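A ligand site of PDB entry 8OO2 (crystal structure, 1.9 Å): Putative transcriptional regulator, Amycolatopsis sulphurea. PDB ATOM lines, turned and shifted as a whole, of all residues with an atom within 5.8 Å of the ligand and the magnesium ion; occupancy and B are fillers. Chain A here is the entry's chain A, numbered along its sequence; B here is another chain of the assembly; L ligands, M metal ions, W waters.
O of Ile 138 sits at hydrogen-bond distance from N2 of the ligand (3.1 Å). An oxygen (O5) of the ligand lies close to a ring nitrogen (NE2) of His 104 (2.9 Å). An oxygen (O7) of the ligand sits at hydrogen-bond distance from the guanidinium group (NH2) of Arg 143 (3.0 Å). The guanidinium group (NH2) of Arg 86 lies within hydrogen-bond range of an oxygen (O1) of the ligand (2.6 Å).
Residues that only touch the magnesium ion: Ser 107 (3.95 Å) and Asp 151 of chain B (3.99 Å). The nearest printed residue that does not touch the magnesium ion is Arg 108 (5.5 Å).
O5 of the ligand is bound to the magnesium ion. Water W2 is bound to the magnesium ion (2.0 Å). The magnesium ion is bound by water W5, 2.1 Å away. Water W6 binds the magnesium ion, at 2.1 Å. The magnesium ion is bound by an oxygen (O6) of the ligand (2.1 Å). The magnesium ion has five donor atoms within binding distance. Slightly farther from the magnesium ion lies a ring nitrogen (NE2) of His 104 (2.7 Å).
Leu 63 touches the ligand. Leu 67 touches the ligand. CD1 of Ile 90 touches C15 of the ligand (3.5 Å). Arg 108 touches the ligand. Pro 109 touches the ligand. Ile 117 touches the ligand (CD1 to C4, 3.7 Å). Leu 120 touches the ligand. Leu 135 touches the ligand (CD1 to C1, 3.8 Å). Ile 139 touches the ligand (CD1 to C20, 3.5 Å). Gly 142 touches the ligand. Asp 151 of chain B touches the ligand (OD2 to O7, 3.9 Å). Hydrophobic or aromatic side chains within 4 Å of the ligand: Leu 63, Leu 67, Ile 90, His 104, Pro 109, Ile 117, Leu 120, Leu 135, Ile 138 and Ile 139. Of the 22 residues printed, 15 come within 4 Å of the ligand.
OD1 of Asp 71 lies within salt-bridge range of NH2 of Arg 86, 2.7 Å away. The side-chain hydroxyl (OG) of Ser 107 is in hydrogen-bond range of the backbone carbonyl oxygen (O) of His 104, at 2.9 Å. The guanidinium group of Arg 108 lies within salt-bridge range of the side-chain carboxylate of Asp 151 of chain B (3.8 Å). The guanidinium group of Arg 143 is in salt-bridge range of the side-chain carboxylate of Asp 151 of chain B (2.7 Å).
Water W5 lies within hydrogen-bond range of the side-chain carboxylate of Asp 151 of chain B (2.8 Å) and a ring nitrogen (NE2) of His 104 (3.5 Å). Water W6 lies within hydrogen-bond range of OD1 of Asp 151 of chain B (2.6 Å) and O of Ser 107 (2.7 Å). Water W2 lies within hydrogen-bond range of OG of Ser 107 (2.9 Å) and NE2 of His 104 (3.5 Å). Water W1 lies within hydrogen-bond range of O3 of the ligand and O of Ile 139. Water W3 lies within hydrogen-bond range of OD2 of Asp 71 (2.7 Å), OD1 of Asp 64 (2.9 Å) and N1 of the ligand (3.1 Å). Water W4 lies within hydrogen-bond range of OD1 of Asp 64 and N1 of the ligand.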
ATOM      1  N   LEU A  63     -15.612 -29.714 -14.986  1.00  0.00           N
ATOM      2  CA  LEU A  63     -14.370 -28.981 -15.220  1.00  0.00           C
ATOM      3  C   LEU A  63     -13.272 -29.403 -14.227  1.00  0.00           C
ATOM      4  O   LEU A  63     -12.074 -29.371 -14.598  1.00  0.00           O
ATOM      5  CB  LEU A  63     -14.659 -27.482 -15.081  1.00  0.00           C
ATOM      6  CG  LEU A  63     -15.451 -26.902 -16.204  1.00  0.00           C
ATOM      7  CD1 LEU A  63     -15.626 -25.322 -16.100  1.00  0.00           C
ATOM      8  CD2 LEU A  63     -14.816 -27.204 -17.599  1.00  0.00           C
ATOM      9  N   ASP A  64     -13.640 -29.715 -12.983  1.00  0.00           N
ATOM     10  CA  ASP A  64     -12.632 -30.185 -12.016  1.00  0.00           C
ATOM     11  C   ASP A  64     -11.817 -31.347 -12.567  1.00  0.00           C
ATOM     12  O   ASP A  64     -10.568 -31.396 -12.418  1.00  0.00           O
ATOM     13  CB  ASP A  64     -13.308 -30.622 -10.714  1.00  0.00           C
ATOM     14  CG  ASP A  64     -13.645 -29.446  -9.825  1.00  0.00           C
ATOM     15  OD1 ASP A  64     -13.390 -28.301 -10.226  1.00  0.00           O
ATOM     16  OD2 ASP A  64     -14.195 -29.728  -8.729  1.00  0.00           O
ATOM     17  N   LEU A  67      -9.319 -29.752 -14.878  1.00  0.00           N
ATOM     18  CA  LEU A  67      -8.458 -28.725 -14.283  1.00  0.00           C
ATOM     19  C   LEU A  67      -7.574 -29.254 -13.175  1.00  0.00           C
ATOM     20  O   LEU A  67      -6.682 -28.528 -12.743  1.00  0.00           O
ATOM     21  CB  LEU A  67      -9.312 -27.570 -13.745  1.00  0.00           C
ATOM     22  CG  LEU A  67     -10.005 -26.746 -14.820  1.00  0.00           C
ATOM     23  CD1 LEU A  67     -11.142 -25.922 -14.211  1.00  0.00           C
ATOM     24  CD2 LEU A  67      -9.017 -25.829 -15.521  1.00  0.00           C
ATOM     25  N   ASP A  71      -4.813 -27.357 -10.921  1.00  0.00           N
ATOM     26  CA  ASP A  71      -5.140 -27.076  -9.534  1.00  0.00           C
ATOM     27  C   ASP A  71      -4.063 -27.594  -8.585  1.00  0.00           C
ATOM     28  O   ASP A  71      -3.908 -27.032  -7.486  1.00  0.00           O
ATOM     29  CB  ASP A  71      -6.470 -27.676  -9.152  1.00  0.00           C
ATOM     30  CG  ASP A  71      -7.663 -26.942  -9.814  1.00  0.00           C
ATOM     31  OD1 ASP A  71      -7.440 -25.918 -10.434  1.00  0.00           O
ATOM     32  OD2 ASP A  71      -8.793 -27.434  -9.680  1.00  0.00           O
ATOM     33  N   LEU A  83      -3.133 -19.175 -16.172  1.00  0.00           N
ATOM     34  CA  LEU A  83      -4.497 -18.761 -16.481  1.00  0.00           C
ATOM     35  C   LEU A  83      -4.864 -19.076 -17.910  1.00  0.00           C
ATOM     36  O   LEU A  83      -5.997 -19.507 -18.186  1.00  0.00           O
ATOM     37  CB  LEU A  83      -4.641 -17.239 -16.244  1.00  0.00           C
ATOM     38  CG  LEU A  83      -5.510 -16.803 -15.077  1.00  0.00           C
ATOM     39  CD1 LEU A  83      -5.614 -15.256 -15.118  1.00  0.00           C
ATOM     40  CD2 LEU A  83      -6.850 -17.432 -15.133  1.00  0.00           C
ATOM     41  N   ARG A  86      -5.681 -22.685 -18.007  1.00  0.00           N
ATOM     42  CA  ARG A  86      -7.015 -22.899 -17.442  1.00  0.00           C
ATOM     43  C   ARG A  86      -8.089 -22.629 -18.506  1.00  0.00           C
ATOM     44  O   ARG A  86      -9.008 -23.453 -18.725  1.00  0.00           O
ATOM     45  CB  ARG A  86      -7.250 -22.011 -16.240  1.00  0.00           C
ATOM     46  CG  ARG A  86      -6.429 -22.370 -15.014  1.00  0.00           C
ATOM     47  CD  ARG A  86      -6.967 -21.662 -13.782  1.00  0.00           C
ATOM     48  NE  ARG A  86      -8.029 -22.425 -13.166  1.00  0.00           N
ATOM     49  CZ  ARG A  86      -7.841 -23.479 -12.399  1.00  0.00           C
ATOM     50  NH1 ARG A  86      -6.598 -23.866 -12.072  1.00  0.00           N
ATOM     51  NH2 ARG A  86      -8.879 -24.141 -11.926  1.00  0.00           N
ATOM     52  N   ALA A  87      -7.970 -21.495 -19.187  1.00  0.00           N
ATOM     53  CA  ALA A  87      -8.975 -21.136 -20.201  1.00  0.00           C
ATOM     54  C   ALA A  87      -8.996 -22.178 -21.320  1.00  0.00           C
ATOM     55  O   ALA A  87     -10.070 -22.627 -21.769  1.00  0.00           O
ATOM     56  CB  ALA A  87      -8.646 -19.767 -20.774  1.00  0.00           C
ATOM     57  N   ILE A  90     -10.693 -25.383 -19.971  1.00  0.00           N
ATOM     58  CA  ILE A  90     -12.144 -25.177 -19.902  1.00  0.00           C
ATOM     59  C   ILE A  90     -12.764 -25.254 -21.293  1.00  0.00           C
ATOM     60  O   ILE A  90     -13.751 -25.993 -21.521  1.00  0.00           O
ATOM     61  CB  ILE A  90     -12.475 -23.824 -19.229  1.00  0.00           C
ATOM     62  CG1 ILE A  90     -12.103 -23.859 -17.758  1.00  0.00           C
ATOM     63  CG2 ILE A  90     -13.954 -23.461 -19.415  1.00  0.00           C
ATOM     64  CD1 ILE A  90     -12.012 -22.455 -17.099  1.00  0.00           C
ATOM     65  N   HIS A 104     -23.241 -25.378 -18.474  1.00  0.00           N
ATOM     66  CA  HIS A 104     -22.418 -24.472 -17.648  1.00  0.00           C
ATOM     67  C   HIS A 104     -23.088 -23.108 -17.501  1.00  0.00           C
ATOM     68  O   HIS A 104     -23.015 -22.571 -16.462  1.00  0.00           O
ATOM     69  CB  HIS A 104     -21.047 -24.359 -18.282  1.00  0.00           C
ATOM     70  CG  HIS A 104     -20.027 -23.775 -17.397  1.00  0.00           C
ATOM     71  ND1 HIS A 104     -19.440 -24.483 -16.371  1.00  0.00           N
ATOM     72  CD2 HIS A 104     -19.493 -22.571 -17.377  1.00  0.00           C
ATOM     73  CE1 HIS A 104     -18.560 -23.711 -15.771  1.00  0.00           C
ATOM     74  NE2 HIS A 104     -18.594 -22.555 -16.365  1.00  0.00           N
ATOM     75  N   SER A 107     -24.295 -21.396 -14.102  1.00  0.00           N
ATOM     76  CA  SER A 107     -23.944 -22.193 -12.909  1.00  0.00           C
ATOM     77  C   SER A 107     -23.083 -21.330 -11.956  1.00  0.00           C
ATOM     78  O   SER A 107     -22.432 -20.367 -12.370  1.00  0.00           O
ATOM     79  CB  SER A 107     -23.191 -23.471 -13.283  1.00  0.00           C
ATOM     80  OG  SER A 107     -21.946 -23.211 -13.897  1.00  0.00           O
ATOM     81  N   ARG A 108     -23.085 -21.728 -10.690  1.00  0.00           N
ATOM     82  CA  ARG A 108     -22.319 -21.040  -9.660  1.00  0.00           C
ATOM     83  C   ARG A 108     -21.685 -22.064  -8.794  1.00  0.00           C
ATOM     84  O   ARG A 108     -22.128 -23.244  -8.743  1.00  0.00           O
ATOM     85  CB  ARG A 108     -23.210 -20.108  -8.839  1.00  0.00           C
ATOM     86  CG  ARG A 108     -23.889 -19.040  -9.632  1.00  0.00           C
ATOM     87  CD  ARG A 108     -22.886 -17.925 -10.083  1.00  0.00           C
ATOM     88  NE  ARG A 108     -23.560 -16.824 -10.723  1.00  0.00           N
ATOM     89  CZ  ARG A 108     -23.741 -16.693 -12.027  1.00  0.00           C
ATOM     90  NH1 ARG A 108     -23.286 -17.588 -12.874  1.00  0.00           N
ATOM     91  NH2 ARG A 108     -24.400 -15.617 -12.489  1.00  0.00           N
ATOM     92  N   PRO A 109     -20.620 -21.733  -8.054  1.00  0.00           N
ATOM     93  CA  PRO A 109     -19.955 -22.699  -7.194  1.00  0.00           C
ATOM     94  C   PRO A 109     -20.916 -23.289  -6.178  1.00  0.00           C
ATOM     95  O   PRO A 109     -21.793 -22.600  -5.666  1.00  0.00           O
ATOM     96  CB  PRO A 109     -18.828 -21.884  -6.502  1.00  0.00           C
ATOM     97  CG  PRO A 109     -18.537 -20.800  -7.502  1.00  0.00           C
ATOM     98  CD  PRO A 109     -19.884 -20.438  -8.119  1.00  0.00           C
ATOM     99  N   ILE A 117     -11.880 -22.034  -3.449  1.00  0.00           N
ATOM    100  CA  ILE A 117     -11.533 -20.800  -4.143  1.00  0.00           C
ATOM    101  C   ILE A 117     -10.259 -20.168  -3.570  1.00  0.00           C
ATOM    102  O   ILE A 117      -9.392 -19.714  -4.342  1.00  0.00           O
ATOM    103  CB  ILE A 117     -12.723 -19.813  -4.095  1.00  0.00           C
ATOM    104  CG1 ILE A 117     -13.862 -20.325  -5.000  1.00  0.00           C
ATOM    105  CG2 ILE A 117     -12.288 -18.400  -4.580  1.00  0.00           C
ATOM    106  CD1 ILE A 117     -15.105 -19.467  -4.930  1.00  0.00           C
ATOM    107  N   LEU A 120      -7.600 -21.757  -5.384  1.00  0.00           N
ATOM    108  CA  LEU A 120      -7.636 -21.358  -6.778  1.00  0.00           C
ATOM    109  C   LEU A 120      -6.972 -20.025  -7.007  1.00  0.00           C
ATOM    110  O   LEU A 120      -6.284 -19.819  -8.004  1.00  0.00           O
ATOM    111  CB  LEU A 120      -9.113 -21.282  -7.245  1.00  0.00           C
ATOM    112  CG  LEU A 120      -9.362 -20.804  -8.658  1.00  0.00           C
ATOM    113  CD1 LEU A 120      -8.757 -21.744  -9.686  1.00  0.00           C
ATOM    114  CD2 LEU A 120     -10.874 -20.676  -8.924  1.00  0.00           C
ATOM    115  N   LEU A 135     -10.602 -13.066  -7.803  1.00  0.00           N
ATOM    116  CA  LEU A 135     -11.849 -13.738  -8.084  1.00  0.00           C
ATOM    117  C   LEU A 135     -12.487 -13.164  -9.351  1.00  0.00           C
ATOM    118  O   LEU A 135     -12.958 -13.904 -10.215  1.00  0.00           O
ATOM    119  CB  LEU A 135     -12.800 -13.594  -6.907  1.00  0.00           C
ATOM    120  CG  LEU A 135     -14.202 -14.189  -7.058  1.00  0.00           C
ATOM    121  CD1 LEU A 135     -14.150 -15.660  -7.332  1.00  0.00           C
ATOM    122  CD2 LEU A 135     -15.023 -13.892  -5.819  1.00  0.00           C
ATOM    123  N   VAL A 137     -10.950 -11.894 -11.821  1.00  0.00           N
ATOM    124  CA  VAL A 137     -10.138 -12.377 -12.919  1.00  0.00           C
ATOM    125  C   VAL A 137     -10.599 -13.769 -13.328  1.00  0.00           C
ATOM    126  O   VAL A 137     -10.846 -14.021 -14.507  1.00  0.00           O
ATOM    127  CB  VAL A 137      -8.656 -12.377 -12.530  1.00  0.00           C
ATOM    128  CG1 VAL A 137      -7.843 -13.239 -13.564  1.00  0.00           C
ATOM    129  CG2 VAL A 137      -8.086 -10.949 -12.471  1.00  0.00           C
ATOM    130  N   ILE A 138     -10.778 -14.667 -12.344  1.00  0.00           N
ATOM    131  CA  ILE A 138     -11.284 -16.017 -12.623  1.00  0.00           C
ATOM    132  C   ILE A 138     -12.626 -15.946 -13.341  1.00  0.00           C
ATOM    133  O   ILE A 138     -12.801 -16.562 -14.377  1.00  0.00           O
ATOM    134  CB  ILE A 138     -11.405 -16.822 -11.320  1.00  0.00           C
ATOM    135  CG1 ILE A 138     -10.025 -17.166 -10.769  1.00  0.00           C
ATOM    136  CG2 ILE A 138     -12.239 -18.084 -11.548  1.00  0.00           C
ATOM    137  CD1 ILE A 138      -9.168 -18.065 -11.654  1.00  0.00           C
ATOM    138  N   ILE A 139     -13.598 -15.212 -12.767  1.00  0.00           N
ATOM    139  CA  ILE A 139     -14.907 -15.106 -13.359  1.00  0.00           C
ATOM    140  C   ILE A 139     -14.799 -14.639 -14.815  1.00  0.00           C
ATOM    141  O   ILE A 139     -15.438 -15.215 -15.716  1.00  0.00           O
ATOM    142  CB  ILE A 139     -15.803 -14.181 -12.543  1.00  0.00           C
ATOM    143  CG1 ILE A 139     -16.078 -14.785 -11.172  1.00  0.00           C
ATOM    144  CG2 ILE A 139     -17.104 -13.918 -13.279  1.00  0.00           C
ATOM    145  CD1 ILE A 139     -16.725 -13.834 -10.190  1.00  0.00           C
ATOM    146  N   ILE A 141     -12.259 -14.640 -16.993  1.00  0.00           N
ATOM    147  CA  ILE A 141     -11.616 -15.573 -17.920  1.00  0.00           C
ATOM    148  C   ILE A 141     -12.568 -16.686 -18.281  1.00  0.00           C
ATOM    149  O   ILE A 141     -12.648 -17.094 -19.451  1.00  0.00           O
ATOM    150  CB  ILE A 141     -10.307 -16.125 -17.327  1.00  0.00           C
ATOM    151  CG1 ILE A 141      -9.256 -15.053 -17.215  1.00  0.00           C
ATOM    152  CG2 ILE A 141      -9.788 -17.319 -18.154  1.00  0.00           C
ATOM    153  CD1 ILE A 141      -8.662 -14.560 -18.514  1.00  0.00           C
ATOM    154  N   GLY A 142     -13.325 -17.194 -17.305  1.00  0.00           N
ATOM    155  CA  GLY A 142     -14.263 -18.276 -17.590  1.00  0.00           C
ATOM    156  C   GLY A 142     -15.427 -17.792 -18.459  1.00  0.00           C
ATOM    157  O   GLY A 142     -15.921 -18.533 -19.302  1.00  0.00           O
ATOM    158  N   ARG A 143     -15.903 -16.588 -18.231  1.00  0.00           N
ATOM    159  CA  ARG A 143     -17.005 -16.044 -19.029  1.00  0.00           C
ATOM    160  C   ARG A 143     -16.541 -15.756 -20.451  1.00  0.00           C
ATOM    161  O   ARG A 143     -17.299 -15.968 -21.383  1.00  0.00           O
ATOM    162  CB  ARG A 143     -17.644 -14.854 -18.360  1.00  0.00           C
ATOM    163  CG  ARG A 143     -18.463 -15.273 -17.137  1.00  0.00           C
ATOM    164  CD  ARG A 143     -19.098 -14.173 -16.381  1.00  0.00           C
ATOM    165  NE  ARG A 143     -19.800 -14.692 -15.244  1.00  0.00           N
ATOM    166  CZ  ARG A 143     -20.311 -14.054 -14.254  1.00  0.00           C
ATOM    167  NH1 ARG A 143     -20.340 -12.708 -14.242  1.00  0.00           N
ATOM    168  NH2 ARG A 143     -20.848 -14.762 -13.244  1.00  0.00           N
ATOM    169  N   ASP B 151     -24.020 -16.029 -18.900  1.00  0.00           N
ATOM    170  CA  ASP B 151     -23.657 -16.550 -17.587  1.00  0.00           C
ATOM    171  C   ASP B 151     -24.278 -15.758 -16.455  1.00  0.00           C
ATOM    172  O   ASP B 151     -24.616 -16.292 -15.397  1.00  0.00           O
ATOM    173  CB  ASP B 151     -22.130 -16.509 -17.412  1.00  0.00           C
ATOM    174  CG  ASP B 151     -21.632 -17.561 -16.430  1.00  0.00           C
ATOM    175  OD1 ASP B 151     -22.262 -18.686 -16.356  1.00  0.00           O
ATOM    176  OD2 ASP B 151     -20.650 -17.236 -15.720  1.00  0.00           O
HETATM  177  N1  LIG L   1     -12.828 -23.842 -11.039  1.00  0.00           N
HETATM  178  C1  LIG L   1     -17.197 -17.526  -8.716  1.00  0.00           C
HETATM  179  C2  LIG L   1     -16.950 -18.410  -9.757  1.00  0.00           C
HETATM  180  C3  LIG L   1     -15.815 -19.412  -9.792  1.00  0.00           C
HETATM  181  C4  LIG L   1     -14.818 -19.576  -8.612  1.00  0.00           C
HETATM  182  C5  LIG L   1     -15.596 -20.343 -10.983  1.00  0.00           C
HETATM  183  C6  LIG L   1     -14.529 -22.421 -12.057  1.00  0.00           C
HETATM  184  C7  LIG L   1     -12.377 -21.257 -13.607  1.00  0.00           C
HETATM  185  C8  LIG L   1     -13.845 -20.916 -13.900  1.00  0.00           C
HETATM  186  C9  LIG L   1     -16.258 -21.075 -13.227  1.00  0.00           C
HETATM  187  C10 LIG L   1     -17.800 -18.430 -11.055  1.00  0.00           C
HETATM  188  C11 LIG L   1     -18.853 -17.410 -10.843  1.00  0.00           C
HETATM  189  C12 LIG L   1     -20.056 -15.559  -9.665  1.00  0.00           C
HETATM  190  C13 LIG L   1     -13.241 -23.189 -12.309  1.00  0.00           C
HETATM  191  C14 LIG L   1     -12.138 -22.320 -12.801  1.00  0.00           C
HETATM  192  C15 LIG L   1     -11.249 -20.527 -14.257  1.00  0.00           C
HETATM  193  C16 LIG L   1     -14.951 -21.849 -13.400  1.00  0.00           C
HETATM  194  C17 LIG L   1     -16.431 -20.259 -12.009  1.00  0.00           C
HETATM  195  C18 LIG L   1     -17.422 -19.329 -11.956  1.00  0.00           C
HETATM  196  C19 LIG L   1     -18.939 -16.603  -9.707  1.00  0.00           C
HETATM  197  C20 LIG L   1     -18.151 -16.726  -8.736  1.00  0.00           C
HETATM  198  C21 LIG L   1     -14.440 -21.367 -11.011  1.00  0.00           C
HETATM  199  N2  LIG L   1     -11.489 -19.288 -14.935  1.00  0.00           N
HETATM  200  O1  LIG L   1     -10.854 -22.575 -12.436  1.00  0.00           O
HETATM  201  O2  LIG L   1     -10.094 -20.948 -14.189  1.00  0.00           O
HETATM  202  O3  LIG L   1     -14.100 -19.800 -14.631  1.00  0.00           O
HETATM  203  O4  LIG L   1     -15.157 -22.839 -14.333  1.00  0.00           O
HETATM  204  O5  LIG L   1     -17.154 -21.098 -14.251  1.00  0.00           O
HETATM  205  O6  LIG L   1     -18.323 -19.242 -13.037  1.00  0.00           O
HETATM  206  O7  LIG L   1     -19.734 -17.273 -11.929  1.00  0.00           O
HETATM  207 MG    MG M   1     -18.994 -20.647 -14.482  1.00  0.00          MG
HETATM  208  O   HOH W   1     -16.269 -17.943 -14.933  1.00  0.00           O
HETATM  209  O   HOH W   2     -19.515 -21.992 -13.041  1.00  0.00           O
HETATM  210  O   HOH W   3     -11.199 -26.377 -10.333  1.00  0.00           O
HETATM  211  O   HOH W   4     -14.805 -26.315 -11.311  1.00  0.00           O
HETATM  212  O   HOH W   5     -18.611 -19.129 -15.869  1.00  0.00           O
HETATM  213  O   HOH W   6     -21.017 -20.082 -14.622  1.00  0.00           O
HETATM  214  O   HOH W   7     -16.880 -25.159 -12.866  1.00  0.00           O
